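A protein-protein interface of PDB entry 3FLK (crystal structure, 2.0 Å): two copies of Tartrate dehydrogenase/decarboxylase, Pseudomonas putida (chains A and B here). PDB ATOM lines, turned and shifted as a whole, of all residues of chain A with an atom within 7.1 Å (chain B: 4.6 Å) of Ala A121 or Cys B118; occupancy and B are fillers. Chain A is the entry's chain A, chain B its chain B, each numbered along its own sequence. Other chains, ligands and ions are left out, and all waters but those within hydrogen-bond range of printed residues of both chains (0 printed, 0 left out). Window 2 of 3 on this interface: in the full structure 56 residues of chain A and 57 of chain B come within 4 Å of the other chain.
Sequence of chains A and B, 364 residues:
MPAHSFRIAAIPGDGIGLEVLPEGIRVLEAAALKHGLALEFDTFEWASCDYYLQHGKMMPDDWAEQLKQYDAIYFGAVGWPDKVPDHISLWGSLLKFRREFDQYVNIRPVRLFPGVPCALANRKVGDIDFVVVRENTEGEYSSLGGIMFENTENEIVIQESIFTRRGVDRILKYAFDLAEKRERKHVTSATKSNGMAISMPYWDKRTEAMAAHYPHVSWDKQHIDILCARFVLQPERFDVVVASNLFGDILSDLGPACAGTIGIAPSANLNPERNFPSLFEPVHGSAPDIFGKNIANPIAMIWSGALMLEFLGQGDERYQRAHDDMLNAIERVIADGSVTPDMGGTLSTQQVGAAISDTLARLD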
ATOM      1  N   CYS A 118      15.186   7.904 -34.378  1.00  0.00           N
ATOM      2  CA  CYS A 118      13.727   7.977 -34.456  1.00  0.00           C
ATOM      3  C   CYS A 118      13.184   8.996 -33.459  1.00  0.00           C
ATOM      4  O   CYS A 118      13.645   9.071 -32.317  1.00  0.00           O
ATOM      5  CB  CYS A 118      13.092   6.604 -34.214  1.00  0.00           C
ATOM      6  SG  CYS A 118      11.281   6.556 -34.398  1.00  0.00           S
ATOM      7  N   ALA A 119      12.207   9.779 -33.907  1.00  0.00           N
ATOM      8  CA  ALA A 119      11.556  10.778 -33.064  1.00  0.00           C
ATOM      9  C   ALA A 119      10.686  10.132 -31.987  1.00  0.00           C
ATOM     10  O   ALA A 119      10.434  10.731 -30.943  1.00  0.00           O
ATOM     11  CB  ALA A 119      10.726  11.719 -33.915  1.00  0.00           C
ATOM     12  N   LEU A 120      10.231   8.911 -32.257  1.00  0.00           N
ATOM     13  CA  LEU A 120       9.367   8.177 -31.339  1.00  0.00           C
ATOM     14  C   LEU A 120      10.170   7.238 -30.445  1.00  0.00           C
ATOM     15  O   LEU A 120      11.129   6.606 -30.895  1.00  0.00           O
ATOM     16  CB  LEU A 120       8.309   7.381 -32.113  1.00  0.00           C
ATOM     17  CG  LEU A 120       7.461   8.099 -33.172  1.00  0.00           C
ATOM     18  CD1 LEU A 120       6.578   7.099 -33.902  1.00  0.00           C
ATOM     19  CD2 LEU A 120       6.619   9.222 -32.572  1.00  0.00           C
ATOM     20  N   ALA A 121       9.769   7.152 -29.180  1.00  0.00           N
ATOM     21  CA  ALA A 121      10.418   6.269 -28.219  1.00  0.00           C
ATOM     22  C   ALA A 121       9.947   4.829 -28.404  1.00  0.00           C
ATOM     23  O   ALA A 121       8.798   4.590 -28.783  1.00  0.00           O
ATOM     24  CB  ALA A 121      10.146   6.740 -26.798  1.00  0.00           C
ATOM     25  N   ASN A 122      10.849   3.882 -28.140  1.00  0.00           N
ATOM     26  CA  ASN A 122      10.555   2.442 -28.196  1.00  0.00           C
ATOM     27  C   ASN A 122      10.062   1.956 -29.564  1.00  0.00           C
ATOM     28  O   ASN A 122       9.174   1.104 -29.650  1.00  0.00           O
ATOM     29  CB  ASN A 122       9.562   2.032 -27.092  1.00  0.00           C
ATOM     30  CG  ASN A 122       9.997   2.485 -25.703  1.00  0.00           C
ATOM     31  OD1 ASN A 122       9.167   2.903 -24.892  1.00  0.00           O
ATOM     32  ND2 ASN A 122      11.299   2.401 -25.421  1.00  0.00           N
ATOM     33  N   ARG A 123      10.641   2.510 -30.627  1.00  0.00           N
ATOM     34  CA  ARG A 123      10.299   2.116 -31.991  1.00  0.00           C
ATOM     35  C   ARG A 123      11.490   1.525 -32.735  1.00  0.00           C
ATOM     36  O   ARG A 123      12.603   2.054 -32.675  1.00  0.00           O
ATOM     37  CB  ARG A 123       9.700   3.292 -32.772  1.00  0.00           C
ATOM     38  CG  ARG A 123       8.202   3.173 -33.050  1.00  0.00           C
ATOM     39  CD  ARG A 123       7.372   3.113 -31.773  1.00  0.00           C
ATOM     40  NE  ARG A 123       6.036   2.572 -32.018  1.00  0.00           N
ATOM     41  CZ  ARG A 123       5.129   2.344 -31.071  1.00  0.00           C
ATOM     42  NH1 ARG A 123       5.402   2.605 -29.798  1.00  0.00           N
ATOM     43  NH2 ARG A 123       3.941   1.851 -31.396  1.00  0.00           N
ATOM     44  N   LYS A 124      11.237   0.421 -33.432  1.00  0.00           N
ATOM     45  CA  LYS A 124      12.259  -0.269 -34.210  1.00  0.00           C
ATOM     46  C   LYS A 124      11.989  -0.112 -35.703  1.00  0.00           C
ATOM     47  O   LYS A 124      10.882   0.259 -36.107  1.00  0.00           O
ATOM     48  CB  LYS A 124      12.301  -1.745 -33.825  1.00  0.00           C
ATOM     49  N   ASP A 127       8.494  -0.698 -37.819  1.00  0.00           N
ATOM     50  CA  ASP A 127       7.323  -0.069 -37.198  1.00  0.00           C
ATOM     51  C   ASP A 127       6.759   1.092 -38.016  1.00  0.00           C
ATOM     52  O   ASP A 127       5.573   1.399 -37.922  1.00  0.00           O
ATOM     53  CB  ASP A 127       7.650   0.412 -35.779  1.00  0.00           C
ATOM     54  CG  ASP A 127       7.861  -0.734 -34.795  1.00  0.00           C
ATOM     55  OD1 ASP A 127       7.755  -1.916 -35.197  1.00  0.00           O
ATOM     56  OD2 ASP A 127       8.131  -0.448 -33.608  1.00  0.00           O
ATOM     57  N   VAL A 232       1.739   8.842 -34.136  1.00  0.00           N
ATOM     58  CA  VAL A 232       2.712   8.999 -33.064  1.00  0.00           C
ATOM     59  C   VAL A 232       2.729   7.793 -32.120  1.00  0.00           C
ATOM     60  O   VAL A 232       3.800   7.337 -31.713  1.00  0.00           O
ATOM     61  CB  VAL A 232       2.454  10.309 -32.268  1.00  0.00           C
ATOM     62  CG1 VAL A 232       3.314  10.383 -31.008  1.00  0.00           C
ATOM     63  CG2 VAL A 232       2.703  11.527 -33.156  1.00  0.00           C
ATOM     64  N   LEU A 233       1.547   7.279 -31.784  1.00  0.00           N
ATOM     65  CA  LEU A 233       1.425   6.242 -30.750  1.00  0.00           C
ATOM     66  C   LEU A 233       1.484   4.806 -31.269  1.00  0.00           C
ATOM     67  O   LEU A 233       2.019   3.927 -30.591  1.00  0.00           O
ATOM     68  CB  LEU A 233       0.160   6.456 -29.908  1.00  0.00           C
ATOM     69  CG  LEU A 233       0.136   7.690 -28.998  1.00  0.00           C
ATOM     70  CD1 LEU A 233      -1.279   7.989 -28.526  1.00  0.00           C
ATOM     71  CD2 LEU A 233       1.078   7.524 -27.812  1.00  0.00           C
ATOM     72  N   LEU B 112       3.176  17.446 -20.529  1.00  0.00           N
ATOM     73  CA  LEU B 112       3.853  16.207 -20.156  1.00  0.00           C
ATOM     74  C   LEU B 112       4.119  16.235 -18.656  1.00  0.00           C
ATOM     75  O   LEU B 112       4.854  17.097 -18.162  1.00  0.00           O
ATOM     76  CB  LEU B 112       5.156  16.017 -20.943  1.00  0.00           C
ATOM     77  CG  LEU B 112       6.082  14.851 -20.562  1.00  0.00           C
ATOM     78  CD1 LEU B 112       5.439  13.487 -20.822  1.00  0.00           C
ATOM     79  CD2 LEU B 112       7.417  14.961 -21.293  1.00  0.00           C
ATOM     80  N   VAL B 116       5.130   9.986 -16.525  1.00  0.00           N
ATOM     81  CA  VAL B 116       4.465   9.541 -17.748  1.00  0.00           C
ATOM     82  C   VAL B 116       5.506   9.032 -18.742  1.00  0.00           C
ATOM     83  O   VAL B 116       6.495   9.723 -19.005  1.00  0.00           O
ATOM     84  CB  VAL B 116       3.643  10.685 -18.418  1.00  0.00           C
ATOM     85  CG1 VAL B 116       3.007  10.213 -19.723  1.00  0.00           C
ATOM     86  CG2 VAL B 116       2.569  11.204 -17.481  1.00  0.00           C
ATOM     87  N   PRO B 117       5.302   7.813 -19.280  1.00  0.00           N
ATOM     88  CA  PRO B 117       6.106   7.369 -20.417  1.00  0.00           C
ATOM     89  C   PRO B 117       5.766   8.200 -21.656  1.00  0.00           C
ATOM     90  O   PRO B 117       4.662   8.087 -22.198  1.00  0.00           O
ATOM     91  CB  PRO B 117       5.680   5.905 -20.607  1.00  0.00           C
ATOM     92  CG  PRO B 117       4.988   5.523 -19.335  1.00  0.00           C
ATOM     93  CD  PRO B 117       4.345   6.779 -18.852  1.00  0.00           C
ATOM     94  N   CYS B 118       6.706   9.041 -22.078  1.00  0.00           N
ATOM     95  CA  CYS B 118       6.511   9.916 -23.234  1.00  0.00           C
ATOM     96  C   CYS B 118       6.600   9.128 -24.540  1.00  0.00           C
ATOM     97  O   CYS B 118       7.397   8.197 -24.663  1.00  0.00           O
ATOM     98  CB  CYS B 118       7.532  11.061 -23.226  1.00  0.00           C
ATOM     99  SG  CYS B 118       7.229  12.375 -24.448  1.00  0.00           S
ATOM    100  N   ALA B 119       5.766   9.511 -25.503  1.00  0.00           N
ATOM    101  CA  ALA B 119       5.751   8.887 -26.821  1.00  0.00           C
ATOM    102  C   ALA B 119       6.956   9.312 -27.656  1.00  0.00           C
ATOM    103  O   ALA B 119       7.348   8.609 -28.590  1.00  0.00           O
ATOM    104  CB  ALA B 119       4.465   9.232 -27.544  1.00  0.00           C
ATOM    105  N   LEU B 120       7.531  10.465 -27.315  1.00  0.00           N
ATOM    106  CA  LEU B 120       8.677  11.017 -28.035  1.00  0.00           C
ATOM    107  C   LEU B 120       9.992  10.624 -27.370  1.00  0.00           C
ATOM    108  O   LEU B 120      10.076  10.537 -26.145  1.00  0.00           O
ATOM    109  CB  LEU B 120       8.579  12.545 -28.121  1.00  0.00           C
ATOM    110  CG  LEU B 120       7.278  13.200 -28.601  1.00  0.00           C
ATOM    111  CD1 LEU B 120       7.409  14.711 -28.547  1.00  0.00           C
ATOM    112  CD2 LEU B 120       6.895  12.744 -30.005  1.00  0.00           C
ATOM    113  N   ALA B 121      11.017  10.399 -28.187  1.00  0.00           N
ATOM    114  CA  ALA B 121      12.339  10.021 -27.693  1.00  0.00           C
ATOM    115  C   ALA B 121      13.078  11.217 -27.096  1.00  0.00           C
ATOM    116  O   ALA B 121      12.821  12.364 -27.471  1.00  0.00           O
ATOM    117  CB  ALA B 121      13.159   9.386 -28.808  1.00  0.00           C
ATOM    118  N   ARG B 123      12.923  13.115 -24.558  1.00  0.00           N
ATOM    119  CA  ARG B 123      12.154  14.269 -24.103  1.00  0.00           C
ATOM    120  C   ARG B 123      11.881  14.172 -22.605  1.00  0.00           C
ATOM    121  O   ARG B 123      11.655  13.080 -22.077  1.00  0.00           O
ATOM    122  CB  ARG B 123      10.838  14.386 -24.879  1.00  0.00           C
ATOM    123  CG  ARG B 123      10.650  15.726 -25.584  1.00  0.00           C
ATOM    124  CD  ARG B 123      11.427  15.746 -26.891  1.00  0.00           C
ATOM    125  NE  ARG B 123      11.791  17.093 -27.326  1.00  0.00           N
ATOM    126  CZ  ARG B 123      12.672  17.354 -28.291  1.00  0.00           C
ATOM    127  NH1 ARG B 123      13.294  16.364 -28.921  1.00  0.00           N
ATOM    128  NH2 ARG B 123      12.941  18.606 -28.627  1.00  0.00           N
ATOM    129  N   ILE B 128       7.205  19.778 -22.962  1.00  0.00           N
ATOM    130  CA  ILE B 128       5.843  19.833 -23.492  1.00  0.00           C
ATOM    131  C   ILE B 128       4.915  20.503 -22.478  1.00  0.00           C
ATOM    132  O   ILE B 128       4.461  19.877 -21.515  1.00  0.00           O
ATOM    133  CB  ILE B 128       5.298  18.435 -23.902  1.00  0.00           C
ATOM    134  CG1 ILE B 128       6.302  17.694 -24.801  1.00  0.00           C
ATOM    135  CG2 ILE B 128       3.933  18.571 -24.590  1.00  0.00           C
ATOM    136  CD1 ILE B 128       5.907  16.266 -25.164  1.00  0.00           C
ATOM    137  N   CYS B 258       1.693  13.184 -28.278  1.00  0.00           N
ATOM    138  CA  CYS B 258       3.130  13.390 -28.108  1.00  0.00           C
ATOM    139  C   CYS B 258       3.502  13.353 -26.629  1.00  0.00           C
ATOM    140  O   CYS B 258       4.567  12.851 -26.262  1.00  0.00           O
ATOM    141  CB  CYS B 258       3.564  14.721 -28.719  1.00  0.00           C
ATOM    142  SG  CYS B 258       3.349  14.835 -30.500  1.00  0.00           S
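Cys A118 touches Ala B121, and with the chains exchanged Ala A121 touches Cys B118. Ala A119 touches Leu B120, and with the chains exchanged Leu A120 touches Ala B119. Ala A119 touches Ala B121, and with the chains exchanged Ala A121 touches Ala B119. Ala B121 touches its own counterpart, Ala A121. Of the 11 pairs that touch across the chains among the printed residues, 9 have their exchanged pair printed and touching as well.
O of Ala A119 lies within hydrogen-bond range of N of Ala B121 (2.8 Å). The backbone carbonyl oxygen of Ala B119 is in hydrogen-bond range of the backbone NH of Ala A121, 2.9 Å away.
Printed residues of chain B that touch a printed residue of chain A: Cys B118, Ala B119, Leu B120 and Ala B121. Hydrophobic or aromatic side chains of chain B that line the printed part of chain A: Ala B119, Leu B120 and Ala B121. Printed residues of chain A that touch a printed residue of chain B: Cys A118, Ala A119, Leu A120, Ala A121, Val A232 and Leu A233. Hydrophobic or aromatic side chains of chain A that line the printed part of chain B: Leu A120, Ala A121, Val A232 and Leu A233. Among the printed residues, 11 pairs touch across the chains. Among the printed residues, no Asp or Glu carboxylate lies within 4 Å of a Lys or Arg side-chain nitrogen of the other chain.
The backbone NH of Leu A120 lies close to the side-chain sulfur of Cys A118 (3.4 Å). NH2 of Arg A123 sits at hydrogen-bond distance from O of Leu A233 (2.9 Å). The backbone NH (N) of Leu B120 sits close to the side-chain sulfur (SG) of Cys B118 (3.5 Å). SG of Cys B118 lies within hydrogen-bond range of O of Cys B258 (3.3 Å).
Among the printed residues, merely in contact across the chains: Cys A118 with Ala B121 (3.6 Å), Ala A119 with Leu B120 (3.4 Å), Leu A120 with Ala B119 (3.4 Å), Leu A120 with Ala B121 (3.98 Å), Ala A121 with Cys B118 (3.8 Å), Ala A121 with Leu B120 (3.9 Å), Ala A121 with Ala B121 (3.6 Å), Val A232 with Ala B119 (3.8 Å) and Leu A233 with Ala B119 (3.8 Å).
Cys B118 touches one residue of chain A. Of the printed residues of chain B, Leu A120 touches Ala B119 (3.4 Å) and Ala B121 (3.98 Å). Of the printed residues of chain A, Ala B121 touches Cys A118 (3.6 Å), Ala A119 (2.8 Å), Leu A120 (3.98 Å) and Ala A121 (3.6 Å). Printed residues of chain A within 4 Å of Ala B119: Leu A120 (3.4 Å), Ala A121 (2.9 Å), Val A232 (3.8 Å) and Leu A233 (3.8 Å). Of the printed residues of chain B, Leu A233 touches Ala B119 (3.8 Å). Arg A123 touches none of the printed residues of chain B. Asp A127 touches none of the printed residues of chain B. The nearest residue of chain A that does not touch Cys B118 is Asn A122 (5.6 Å).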
